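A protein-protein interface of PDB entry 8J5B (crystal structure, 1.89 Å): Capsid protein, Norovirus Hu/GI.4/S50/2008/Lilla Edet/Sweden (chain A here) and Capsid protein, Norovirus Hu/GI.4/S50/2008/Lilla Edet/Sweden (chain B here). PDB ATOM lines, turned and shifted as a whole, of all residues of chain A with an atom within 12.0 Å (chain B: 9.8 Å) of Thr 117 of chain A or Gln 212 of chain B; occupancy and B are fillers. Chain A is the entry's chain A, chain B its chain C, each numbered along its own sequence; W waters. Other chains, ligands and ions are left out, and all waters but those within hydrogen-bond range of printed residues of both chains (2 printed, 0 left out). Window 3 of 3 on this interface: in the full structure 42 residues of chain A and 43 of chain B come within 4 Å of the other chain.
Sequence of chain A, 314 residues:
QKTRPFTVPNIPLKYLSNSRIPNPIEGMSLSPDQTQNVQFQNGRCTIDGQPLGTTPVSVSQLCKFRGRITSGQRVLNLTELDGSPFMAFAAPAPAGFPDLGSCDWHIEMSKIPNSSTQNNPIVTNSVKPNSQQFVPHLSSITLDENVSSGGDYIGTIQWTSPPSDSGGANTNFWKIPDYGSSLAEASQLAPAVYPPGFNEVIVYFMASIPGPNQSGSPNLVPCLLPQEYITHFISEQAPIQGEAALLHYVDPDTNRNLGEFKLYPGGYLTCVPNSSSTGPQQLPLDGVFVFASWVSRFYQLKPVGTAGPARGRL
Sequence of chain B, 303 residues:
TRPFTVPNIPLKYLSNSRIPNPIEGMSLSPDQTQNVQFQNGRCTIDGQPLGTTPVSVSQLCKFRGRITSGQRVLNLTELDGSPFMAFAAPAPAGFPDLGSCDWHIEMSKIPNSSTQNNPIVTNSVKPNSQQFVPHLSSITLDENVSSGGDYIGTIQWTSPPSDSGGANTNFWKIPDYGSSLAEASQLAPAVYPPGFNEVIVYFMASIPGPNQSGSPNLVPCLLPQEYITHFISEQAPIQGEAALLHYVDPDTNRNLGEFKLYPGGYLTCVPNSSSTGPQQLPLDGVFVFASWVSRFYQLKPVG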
ATOM      1  N   LYS A 111     -19.632 -17.820  23.535  1.00  0.00           N
ATOM      2  CA  LYS A 111     -20.071 -16.450  23.860  1.00  0.00           C
ATOM      3  C   LYS A 111     -20.883 -15.899  22.686  1.00  0.00           C
ATOM      4  O   LYS A 111     -20.507 -16.153  21.520  1.00  0.00           O
ATOM      5  CB  LYS A 111     -18.870 -15.556  24.175  1.00  0.00           C
ATOM      6  CG  LYS A 111     -18.497 -15.525  25.643  1.00  0.00           C
ATOM      7  CD  LYS A 111     -17.352 -14.591  25.934  1.00  0.00           C
ATOM      8  CE  LYS A 111     -16.011 -15.285  25.956  1.00  0.00           C
ATOM      9  NZ  LYS A 111     -14.966 -14.330  26.388  1.00  0.00           N
ATOM     10  N   PRO A 113     -22.775 -12.072  21.591  1.00  0.00           N
ATOM     11  CA  PRO A 113     -22.466 -12.346  20.186  1.00  0.00           C
ATOM     12  C   PRO A 113     -20.965 -12.630  20.039  1.00  0.00           C
ATOM     13  O   PRO A 113     -20.254 -12.456  20.990  1.00  0.00           O
ATOM     14  CB  PRO A 113     -22.925 -11.038  19.523  1.00  0.00           C
ATOM     15  CG  PRO A 113     -22.542  -9.963  20.532  1.00  0.00           C
ATOM     16  CD  PRO A 113     -22.698 -10.631  21.892  1.00  0.00           C
ATOM     17  N   ASN A 114     -20.528 -13.103  18.874  1.00  0.00           N
ATOM     18  CA  ASN A 114     -19.090 -13.212  18.556  1.00  0.00           C
ATOM     19  C   ASN A 114     -18.480 -11.807  18.615  1.00  0.00           C
ATOM     20  O   ASN A 114     -19.125 -10.886  18.078  1.00  0.00           O
ATOM     21  CB  ASN A 114     -18.868 -13.794  17.168  1.00  0.00           C
ATOM     22  CG  ASN A 114     -17.430 -13.633  16.730  1.00  0.00           C
ATOM     23  OD1 ASN A 114     -16.557 -14.383  17.171  1.00  0.00           O
ATOM     24  ND2 ASN A 114     -17.189 -12.661  15.863  1.00  0.00           N
ATOM     25  N   SER A 115     -17.305 -11.647  19.235  1.00  0.00           N
ATOM     26  CA  SER A 115     -16.451 -10.429  19.102  1.00  0.00           C
ATOM     27  C   SER A 115     -15.043 -10.816  18.638  1.00  0.00           C
ATOM     28  O   SER A 115     -14.178  -9.922  18.600  1.00  0.00           O
ATOM     29  CB  SER A 115     -16.365  -9.663  20.385  1.00  0.00           C
ATOM     30  OG  SER A 115     -15.749 -10.468  21.377  1.00  0.00           O
ATOM     31  N   SER A 116     -14.817 -12.091  18.303  1.00  0.00           N
ATOM     32  CA  SER A 116     -13.465 -12.668  18.102  1.00  0.00           C
ATOM     33  C   SER A 116     -13.082 -12.586  16.618  1.00  0.00           C
ATOM     34  O   SER A 116     -13.996 -12.520  15.760  1.00  0.00           O
ATOM     35  CB  SER A 116     -13.423 -14.083  18.633  1.00  0.00           C
ATOM     36  OG  SER A 116     -14.213 -14.940  17.815  1.00  0.00           O
ATOM     37  N   THR A 117     -11.778 -12.548  16.333  1.00  0.00           N
ATOM     38  CA  THR A 117     -11.196 -12.462  14.969  1.00  0.00           C
ATOM     39  C   THR A 117     -10.351 -13.707  14.665  1.00  0.00           C
ATOM     40  O   THR A 117      -9.945 -13.860  13.496  1.00  0.00           O
ATOM     41  CB  THR A 117     -10.371 -11.172  14.772  1.00  0.00           C
ATOM     42  OG1 THR A 117      -9.436 -11.010  15.838  1.00  0.00           O
ATOM     43  CG2 THR A 117     -11.219  -9.923  14.691  1.00  0.00           C
ATOM     44  N   GLN A 118     -10.101 -14.564  15.661  1.00  0.00           N
ATOM     45  CA  GLN A 118      -9.321 -15.833  15.537  1.00  0.00           C
ATOM     46  C   GLN A 118      -9.719 -16.759  16.692  1.00  0.00           C
ATOM     47  O   GLN A 118     -10.530 -16.357  17.513  1.00  0.00           O
ATOM     48  CB  GLN A 118      -7.821 -15.522  15.573  1.00  0.00           C
ATOM     49  CG  GLN A 118      -7.460 -14.628  16.751  1.00  0.00           C
ATOM     50  CD  GLN A 118      -6.060 -14.071  16.706  1.00  0.00           C
ATOM     51  OE1 GLN A 118      -5.247 -14.444  15.861  1.00  0.00           O
ATOM     52  NE2 GLN A 118      -5.764 -13.187  17.648  1.00  0.00           N
ATOM     53  N   ASN A 119      -9.118 -17.941  16.770  1.00  0.00           N
ATOM     54  CA  ASN A 119      -9.289 -18.898  17.895  1.00  0.00           C
ATOM     55  C   ASN A 119     -10.643 -19.605  17.738  1.00  0.00           C
ATOM     56  O   ASN A 119     -11.560 -19.076  17.046  1.00  0.00           O
ATOM     57  CB  ASN A 119      -9.190 -18.254  19.281  1.00  0.00           C
ATOM     58  CG  ASN A 119      -7.915 -17.466  19.507  1.00  0.00           C
ATOM     59  OD1 ASN A 119      -7.949 -16.318  19.947  1.00  0.00           O
ATOM     60  ND2 ASN A 119      -6.782 -18.075  19.207  1.00  0.00           N
ATOM     61  N   ASN A 120     -10.751 -20.734  18.414  1.00  0.00           N
ATOM     62  CA  ASN A 120     -11.974 -21.554  18.513  1.00  0.00           C
ATOM     63  C   ASN A 120     -12.815 -20.950  19.626  1.00  0.00           C
ATOM     64  O   ASN A 120     -12.325 -20.716  20.721  1.00  0.00           O
ATOM     65  CB  ASN A 120     -11.614 -23.011  18.772  1.00  0.00           C
ATOM     66  CG  ASN A 120     -12.819 -23.926  18.805  1.00  0.00           C
ATOM     67  OD1 ASN A 120     -13.928 -23.504  19.119  1.00  0.00           O
ATOM     68  ND2 ASN A 120     -12.578 -25.188  18.516  1.00  0.00           N
ATOM     69  N   PRO A 121     -14.091 -20.605  19.364  1.00  0.00           N
ATOM     70  CA  PRO A 121     -14.956 -20.067  20.411  1.00  0.00           C
ATOM     71  C   PRO A 121     -15.653 -21.115  21.284  1.00  0.00           C
ATOM     72  O   PRO A 121     -16.305 -20.724  22.194  1.00  0.00           O
ATOM     73  CB  PRO A 121     -16.002 -19.306  19.574  1.00  0.00           C
ATOM     74  CG  PRO A 121     -16.151 -20.140  18.339  1.00  0.00           C
ATOM     75  CD  PRO A 121     -14.755 -20.661  18.050  1.00  0.00           C
ATOM     76  N   ILE A 122     -15.552 -22.405  20.960  1.00  0.00           N
ATOM     77  CA  ILE A 122     -16.330 -23.450  21.682  1.00  0.00           C
ATOM     78  C   ILE A 122     -15.615 -23.738  23.000  1.00  0.00           C
ATOM     79  O   ILE A 122     -14.412 -24.046  22.984  1.00  0.00           O
ATOM     80  CB  ILE A 122     -16.554 -24.725  20.849  1.00  0.00           C
ATOM     81  CG1 ILE A 122     -17.117 -24.427  19.458  1.00  0.00           C
ATOM     82  CG2 ILE A 122     -17.468 -25.689  21.595  1.00  0.00           C
ATOM     83  CD1 ILE A 122     -18.508 -23.881  19.476  1.00  0.00           C
ATOM     84  N   SER B 100     -18.319 -19.307   1.388  1.00  0.00           N
ATOM     85  CA  SER B 100     -17.202 -18.386   1.763  1.00  0.00           C
ATOM     86  C   SER B 100     -16.866 -18.515   3.251  1.00  0.00           C
ATOM     87  O   SER B 100     -16.966 -17.495   3.972  1.00  0.00           O
ATOM     88  CB  SER B 100     -17.526 -16.956   1.414  1.00  0.00           C
ATOM     89  OG  SER B 100     -16.530 -16.054   1.913  1.00  0.00           O
ATOM     90  N   TRP B 157     -18.552 -24.607  14.426  1.00  0.00           N
ATOM     91  CA  TRP B 157     -18.158 -23.183  14.282  1.00  0.00           C
ATOM     92  C   TRP B 157     -17.620 -22.921  12.865  1.00  0.00           C
ATOM     93  O   TRP B 157     -17.331 -23.884  12.159  1.00  0.00           O
ATOM     94  CB  TRP B 157     -17.210 -22.741  15.415  1.00  0.00           C
ATOM     95  CG  TRP B 157     -15.913 -23.484  15.553  1.00  0.00           C
ATOM     96  CD1 TRP B 157     -15.719 -24.725  16.102  1.00  0.00           C
ATOM     97  CD2 TRP B 157     -14.604 -22.982  15.221  1.00  0.00           C
ATOM     98  NE1 TRP B 157     -14.387 -25.044  16.095  1.00  0.00           N
ATOM     99  CE2 TRP B 157     -13.678 -23.990  15.566  1.00  0.00           C
ATOM    100  CE3 TRP B 157     -14.121 -21.790  14.655  1.00  0.00           C
ATOM    101  CZ2 TRP B 157     -12.311 -23.835  15.339  1.00  0.00           C
ATOM    102  CZ3 TRP B 157     -12.771 -21.643  14.425  1.00  0.00           C
ATOM    103  CH2 TRP B 157     -11.879 -22.656  14.765  1.00  0.00           C
ATOM    104  N   THR B 158     -17.545 -21.653  12.448  1.00  0.00           N
ATOM    105  CA  THR B 158     -17.098 -21.251  11.099  1.00  0.00           C
ATOM    106  C   THR B 158     -15.915 -20.294  11.287  1.00  0.00           C
ATOM    107  O   THR B 158     -15.762 -19.718  12.399  1.00  0.00           O
ATOM    108  CB  THR B 158     -18.225 -20.601  10.277  1.00  0.00           C
ATOM    109  OG1 THR B 158     -18.442 -19.324  10.855  1.00  0.00           O
ATOM    110  CG2 THR B 158     -19.523 -21.388  10.238  1.00  0.00           C
ATOM    111  N   SER B 159     -15.075 -20.184  10.271  1.00  0.00           N
ATOM    112  CA  SER B 159     -13.955 -19.209  10.231  1.00  0.00           C
ATOM    113  C   SER B 159     -13.815 -18.709   8.794  1.00  0.00           C
ATOM    114  O   SER B 159     -14.344 -19.324   7.861  1.00  0.00           O
ATOM    115  CB  SER B 159     -12.676 -19.815  10.813  1.00  0.00           C
ATOM    116  OG  SER B 159     -12.112 -20.818   9.988  1.00  0.00           O
ATOM    117  N   PRO B 160     -13.111 -17.581   8.565  1.00  0.00           N
ATOM    118  CA  PRO B 160     -12.868 -17.100   7.208  1.00  0.00           C
ATOM    119  C   PRO B 160     -12.264 -18.223   6.367  1.00  0.00           C
ATOM    120  O   PRO B 160     -11.553 -19.065   6.915  1.00  0.00           O
ATOM    121  CB  PRO B 160     -11.855 -15.946   7.389  1.00  0.00           C
ATOM    122  CG  PRO B 160     -12.007 -15.518   8.830  1.00  0.00           C
ATOM    123  CD  PRO B 160     -12.439 -16.759   9.584  1.00  0.00           C
ATOM    124  N   PRO B 161     -12.499 -18.260   5.030  1.00  0.00           N
ATOM    125  CA  PRO B 161     -12.125 -19.412   4.204  1.00  0.00           C
ATOM    126  C   PRO B 161     -10.619 -19.448   3.910  1.00  0.00           C
ATOM    127  O   PRO B 161     -10.034 -18.390   3.691  1.00  0.00           O
ATOM    128  CB  PRO B 161     -12.942 -19.228   2.913  1.00  0.00           C
ATOM    129  CG  PRO B 161     -13.126 -17.720   2.805  1.00  0.00           C
ATOM    130  CD  PRO B 161     -13.122 -17.190   4.231  1.00  0.00           C
ATOM    131  N   SER B 162     -10.031 -20.647   3.970  1.00  0.00           N
ATOM    132  CA  SER B 162      -8.609 -20.919   3.648  1.00  0.00           C
ATOM    133  C   SER B 162      -8.408 -20.785   2.138  1.00  0.00           C
ATOM    134  O   SER B 162      -9.400 -20.814   1.391  1.00  0.00           O
ATOM    135  CB  SER B 162      -8.188 -22.283   4.134  1.00  0.00           C
ATOM    136  OG  SER B 162      -8.295 -22.367   5.545  1.00  0.00           O
ATOM    137  N   SER B 164      -8.023 -18.566   0.087  1.00  0.00           N
ATOM    138  CA  SER B 164      -9.025 -17.622  -0.466  1.00  0.00           C
ATOM    139  C   SER B 164      -8.420 -16.226  -0.659  1.00  0.00           C
ATOM    140  O   SER B 164      -9.170 -15.325  -1.076  1.00  0.00           O
ATOM    141  CB  SER B 164     -10.226 -17.571   0.432  1.00  0.00           C
ATOM    142  OG  SER B 164      -9.911 -16.902   1.636  1.00  0.00           O
ATOM    143  N   GLY B 165      -7.115 -16.075  -0.404  1.00  0.00           N
ATOM    144  CA  GLY B 165      -6.416 -14.777  -0.385  1.00  0.00           C
ATOM    145  C   GLY B 165      -7.019 -13.850   0.655  1.00  0.00           C
ATOM    146  O   GLY B 165      -7.290 -12.674   0.313  1.00  0.00           O
ATOM    147  N   GLY B 166      -7.269 -14.383   1.858  1.00  0.00           N
ATOM    148  CA  GLY B 166      -7.659 -13.618   3.058  1.00  0.00           C
ATOM    149  C   GLY B 166      -9.057 -13.026   2.980  1.00  0.00           C
ATOM    150  O   GLY B 166      -9.281 -12.001   3.640  1.00  0.00           O
ATOM    151  N   ALA B 167      -9.981 -13.689   2.275  1.00  0.00           N
ATOM    152  CA  ALA B 167     -11.403 -13.300   2.154  1.00  0.00           C
ATOM    153  C   ALA B 167     -12.075 -13.535   3.509  1.00  0.00           C
ATOM    154  O   ALA B 167     -11.647 -14.439   4.261  1.00  0.00           O
ATOM    155  CB  ALA B 167     -12.092 -14.059   1.041  1.00  0.00           C
ATOM    156  N   ASN B 168     -13.047 -12.686   3.842  1.00  0.00           N
ATOM    157  CA  ASN B 168     -13.799 -12.798   5.110  1.00  0.00           C
ATOM    158  C   ASN B 168     -14.824 -13.921   4.959  1.00  0.00           C
ATOM    159  O   ASN B 168     -15.098 -14.345   3.815  1.00  0.00           O
ATOM    160  CB  ASN B 168     -14.489 -11.489   5.484  1.00  0.00           C
ATOM    161  CG  ASN B 168     -14.818 -11.405   6.958  1.00  0.00           C
ATOM    162  OD1 ASN B 168     -14.403 -12.248   7.757  1.00  0.00           O
ATOM    163  ND2 ASN B 168     -15.531 -10.361   7.335  1.00  0.00           N
ATOM    164  N   THR B 169     -15.336 -14.395   6.091  1.00  0.00           N
ATOM    165  CA  THR B 169     -16.638 -15.092   6.167  1.00  0.00           C
ATOM    166  C   THR B 169     -17.642 -14.277   5.355  1.00  0.00           C
ATOM    167  O   THR B 169     -17.616 -13.039   5.479  1.00  0.00           O
ATOM    168  CB  THR B 169     -17.081 -15.218   7.624  1.00  0.00           C
ATOM    169  OG1 THR B 169     -16.084 -16.052   8.200  1.00  0.00           O
ATOM    170  CG2 THR B 169     -18.452 -15.835   7.798  1.00  0.00           C
ATOM    171  N   ASN B 170     -18.458 -14.941   4.534  1.00  0.00           N
ATOM    172  CA  ASN B 170     -19.503 -14.293   3.700  1.00  0.00           C
ATOM    173  C   ASN B 170     -20.656 -15.280   3.487  1.00  0.00           C
ATOM    174  O   ASN B 170     -20.656 -16.018   2.461  1.00  0.00           O
ATOM    175  CB  ASN B 170     -18.970 -13.777   2.362  1.00  0.00           C
ATOM    176  CG  ASN B 170     -20.048 -13.042   1.595  1.00  0.00           C
ATOM    177  OD1 ASN B 170     -21.170 -12.939   2.075  1.00  0.00           O
ATOM    178  ND2 ASN B 170     -19.732 -12.559   0.406  1.00  0.00           N
ATOM    179  N   GLY B 209     -18.133 -18.607  15.585  1.00  0.00           N
ATOM    180  CA  GLY B 209     -16.993 -18.531  14.663  1.00  0.00           C
ATOM    181  C   GLY B 209     -16.396 -17.133  14.700  1.00  0.00           C
ATOM    182  O   GLY B 209     -17.124 -16.155  14.833  1.00  0.00           O
ATOM    183  N   PRO B 210     -15.068 -16.985  14.575  1.00  0.00           N
ATOM    184  CA  PRO B 210     -14.472 -15.658  14.408  1.00  0.00           C
ATOM    185  C   PRO B 210     -14.734 -15.112  12.997  1.00  0.00           C
ATOM    186  O   PRO B 210     -15.174 -15.860  12.134  1.00  0.00           O
ATOM    187  CB  PRO B 210     -12.984 -15.934  14.575  1.00  0.00           C
ATOM    188  CG  PRO B 210     -12.848 -17.334  14.032  1.00  0.00           C
ATOM    189  CD  PRO B 210     -14.080 -18.070  14.523  1.00  0.00           C
ATOM    190  N   ASN B 211     -14.510 -13.820  12.806  1.00  0.00           N
ATOM    191  CA  ASN B 211     -14.485 -13.176  11.468  1.00  0.00           C
ATOM    192  C   ASN B 211     -13.585 -11.936  11.550  1.00  0.00           C
ATOM    193  O   ASN B 211     -13.099 -11.619  12.656  1.00  0.00           O
ATOM    194  CB  ASN B 211     -15.886 -12.876  10.929  1.00  0.00           C
ATOM    195  CG  ASN B 211     -16.769 -12.116  11.894  1.00  0.00           C
ATOM    196  OD1 ASN B 211     -16.364 -11.106  12.470  1.00  0.00           O
ATOM    197  ND2 ASN B 211     -17.994 -12.593  12.051  1.00  0.00           N
ATOM    198  N   GLN B 212     -13.349 -11.287  10.410  1.00  0.00           N
ATOM    199  CA  GLN B 212     -12.269 -10.281  10.273  1.00  0.00           C
ATOM    200  C   GLN B 212     -12.589  -9.008  11.063  1.00  0.00           C
ATOM    201  O   GLN B 212     -11.624  -8.341  11.454  1.00  0.00           O
ATOM    202  CB  GLN B 212     -11.985 -10.040   8.790  1.00  0.00           C
ATOM    203  CG  GLN B 212     -11.127 -11.162   8.215  1.00  0.00           C
ATOM    204  CD  GLN B 212     -11.047 -11.088   6.714  1.00  0.00           C
ATOM    205  OE1 GLN B 212     -11.707 -10.261   6.090  1.00  0.00           O
ATOM    206  NE2 GLN B 212     -10.243 -11.959   6.134  1.00  0.00           N
ATOM    207  N   SER B 213     -13.870  -8.700  11.314  1.00  0.00           N
ATOM    208  CA  SER B 213     -14.331  -7.455  11.981  1.00  0.00           C
ATOM    209  C   SER B 213     -14.594  -7.681  13.475  1.00  0.00           C
ATOM    210  O   SER B 213     -14.864  -6.685  14.173  1.00  0.00           O
ATOM    211  CB  SER B 213     -15.570  -6.929  11.316  1.00  0.00           C
ATOM    212  OG  SER B 213     -15.563  -7.254   9.942  1.00  0.00           O
ATOM    213  N   GLY B 214     -14.572  -8.931  13.948  1.00  0.00           N
ATOM    214  CA  GLY B 214     -14.877  -9.253  15.357  1.00  0.00           C
ATOM    215  C   GLY B 214     -16.307  -8.856  15.678  1.00  0.00           C
ATOM    216  O   GLY B 214     -16.517  -8.186  16.725  1.00  0.00           O
ATOM    217  N   SER B 215     -17.228  -9.272  14.788  1.00  0.00           N
ATOM    218  CA  SER B 215     -18.656  -8.884  14.704  1.00  0.00           C
ATOM    219  C   SER B 215     -19.542 -10.124  14.778  1.00  0.00           C
ATOM    220  O   SER B 215     -19.082 -11.251  14.584  1.00  0.00           O
ATOM    221  CB  SER B 215     -18.920  -8.124  13.436  1.00  0.00           C
ATOM    222  OG  SER B 215     -18.651  -8.926  12.292  1.00  0.00           O
ATOM    223  N   PRO B 216     -20.847  -9.945  15.066  1.00  0.00           N
ATOM    224  CA  PRO B 216     -21.784 -11.061  15.089  1.00  0.00           C
ATOM    225  C   PRO B 216     -21.682 -11.890  13.807  1.00  0.00           C
ATOM    226  O   PRO B 216     -21.646 -11.381  12.697  1.00  0.00           O
ATOM    227  CB  PRO B 216     -23.153 -10.388  15.243  1.00  0.00           C
ATOM    228  CG  PRO B 216     -22.819  -9.133  15.989  1.00  0.00           C
ATOM    229  CD  PRO B 216     -21.507  -8.668  15.389  1.00  0.00           C
ATOM    230  N   ASN B 217     -21.655 -13.188  14.010  1.00  0.00           N
ATOM    231  CA  ASN B 217     -21.478 -14.189  12.947  1.00  0.00           C
ATOM    232  C   ASN B 217     -22.869 -14.644  12.471  1.00  0.00           C
ATOM    233  O   ASN B 217     -23.288 -15.763  12.840  1.00  0.00           O
ATOM    234  CB  ASN B 217     -20.557 -15.274  13.496  1.00  0.00           C
ATOM    235  CG  ASN B 217     -19.901 -16.066  12.401  1.00  0.00           C
ATOM    236  OD1 ASN B 217     -19.230 -15.484  11.558  1.00  0.00           O
ATOM    237  ND2 ASN B 217     -20.093 -17.384  12.423  1.00  0.00           N
HETATM  238  O   HOH W   1     -18.068 -16.933  18.047  1.00  0.00           O
HETATM  239  O   HOH W   2     -22.446 -13.798  16.602  1.00  0.00           O
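OD1 of Asn 114 of chain A lies close to O of Gly 209 of chain B, at 3.0 Å. The side-chain amide nitrogen of Asn 114 of chain A lies within hydrogen-bond range of the backbone carbonyl oxygen of Ser 215 of chain B. The backbone NH (N) of Asn 211 of chain B lies within hydrogen-bond range of the backbone carbonyl oxygen (O) of Ser 116 of chain A (3.3 Å). ND2 of Asn 120 of chain A lies close to NE1 of Trp 157 of chain B (3.0 Å). The backbone carbonyl oxygen (O) of Ser 115 of chain A sits close to the backbone carbonyl oxygen (O) of Gly 214 of chain B, 3.5 Å away.
N of Ile 122 of chain A sits at hydrogen-bond distance from OD1 of Asn 120 of chain A (2.7 Å). The backbone carbonyl oxygen (O) of Gly 166 of chain B lies within hydrogen-bond range of the side-chain amide nitrogen (NE2) of Gln 212 of chain B, 2.7 Å away. OD1 of Asn 168 of chain B sits at hydrogen-bond distance from N of Gln 212 of chain B (3.0 Å). The backbone NH (N) of Gly 214 of chain B sits at hydrogen-bond distance from the side-chain amide oxygen (OD1) of Asn 211 of chain B (3.2 Å). The backbone carbonyl oxygen (O) of Ser 215 of chain B lies within hydrogen-bond range of the side-chain amide nitrogen (ND2) of Asn 211 of chain B, 3.1 Å away. OD1 of Asn 217 of chain B is in hydrogen-bond range of ND2 of Asn 211 of chain B (3.2 Å).
Asn 114 of chain A touches Pro 210 of chain B (OD1 to CA, 3.7 Å). Asn 211 of chain B touches Asn 114 of chain A. O of Asn 114 of chain A touches N of Pro 216 of chain B, at 3.6 Å. Ser 116 of chain A touches Pro 210 of chain B. Ser 116 of chain A touches Gly 214 of chain B. Thr 117 of chain A touches Gln 212 of chain B (CG2 to O, 3.6 Å). Trp 157 of chain B touches Asn 119 of chain A (CZ3 to O, 3.9 Å). Asn 119 of chain A touches Pro 210 of chain B (O to CD, 3.7 Å). Pro 121 of chain A touches Trp 157 of chain B. Ile 122 of chain A touches Trp 157 of chain B.
Printed residues of chain B within 4 Å of Ser 115 of chain A: Gly 214 (3.3 Å). Of chain B, only Pro 210 (3.4 Å), Asn 211 (3.1 Å), Gln 212 (3.6 Å) and Gly 214 (3.6 Å) come within 4 Å of Thr 117 of chain A. Of the printed residues of chain B, Pro 121 of chain A touches Trp 157 and Gly 209. Thr 158 of chain B touches none of the printed residues of chain A. No residue of chain A comes within 4 Å of Pro 160 of chain B. Gly 165 of chain B touches none of the printed residues of chain A. No residue of chain A comes within 4 Å of Gly 166 of chain B. Printed residues of chain A within 4 Å of Gly 209 of chain B: Asn 114 and Pro 121. Pro 210 of chain B touches just these residues of chain A: Asn 114 (3.7 Å), Ser 116 (3.4 Å), Thr 117 (3.4 Å), Gln 118 (3.4 Å) and Asn 119 (3.7 Å). Of chain A, only Asn 114, Ser 116 and Thr 117 come within 4 Å of Asn 211 of chain B. Of chain A, only Thr 117 comes within 4 Å of Gln 212 of chain B. No residue of chain A comes within 4 Å of Ser 213 of chain B. Of chain A, only Asn 114 (3.9 Å), Ser 115 (3.3 Å), Ser 116 (3.4 Å) and Thr 117 (3.6 Å) come within 4 Å of Gly 214 of chain B. Printed residues of chain A within 4 Å of Ser 215 of chain B: Asn 114. Of the printed residues of chain A, Pro 216 of chain B touches Asn 114 (3.6 Å).
Printed residues of chain B that touch a printed residue of chain A: Trp 157, Gly 209, Pro 210, Asn 211, Gln 212, Gly 214, Ser 215 and Pro 216. Hydrophobic or aromatic side chains of chain B within 4 Å of the printed part of chain A: Trp 157 and Pro 210. Of the 11 printed residues of chain A, 9 touch a printed residue of chain B. Among the printed residues, no Asp or Glu carboxylate lies within 4 Å of a Lys or Arg side-chain nitrogen of the other chain.
Water W2 lies within hydrogen-bond range of N of Asn 217 of chain B (2.8 Å) and N of Asn 114 of chain A (3.1 Å). Water W1 lies within hydrogen-bond range of the backbone NH of Gly 209 of chain B (3.0 Å) and the side-chain amide oxygen of Asn 114 of chain A (3.1 Å).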
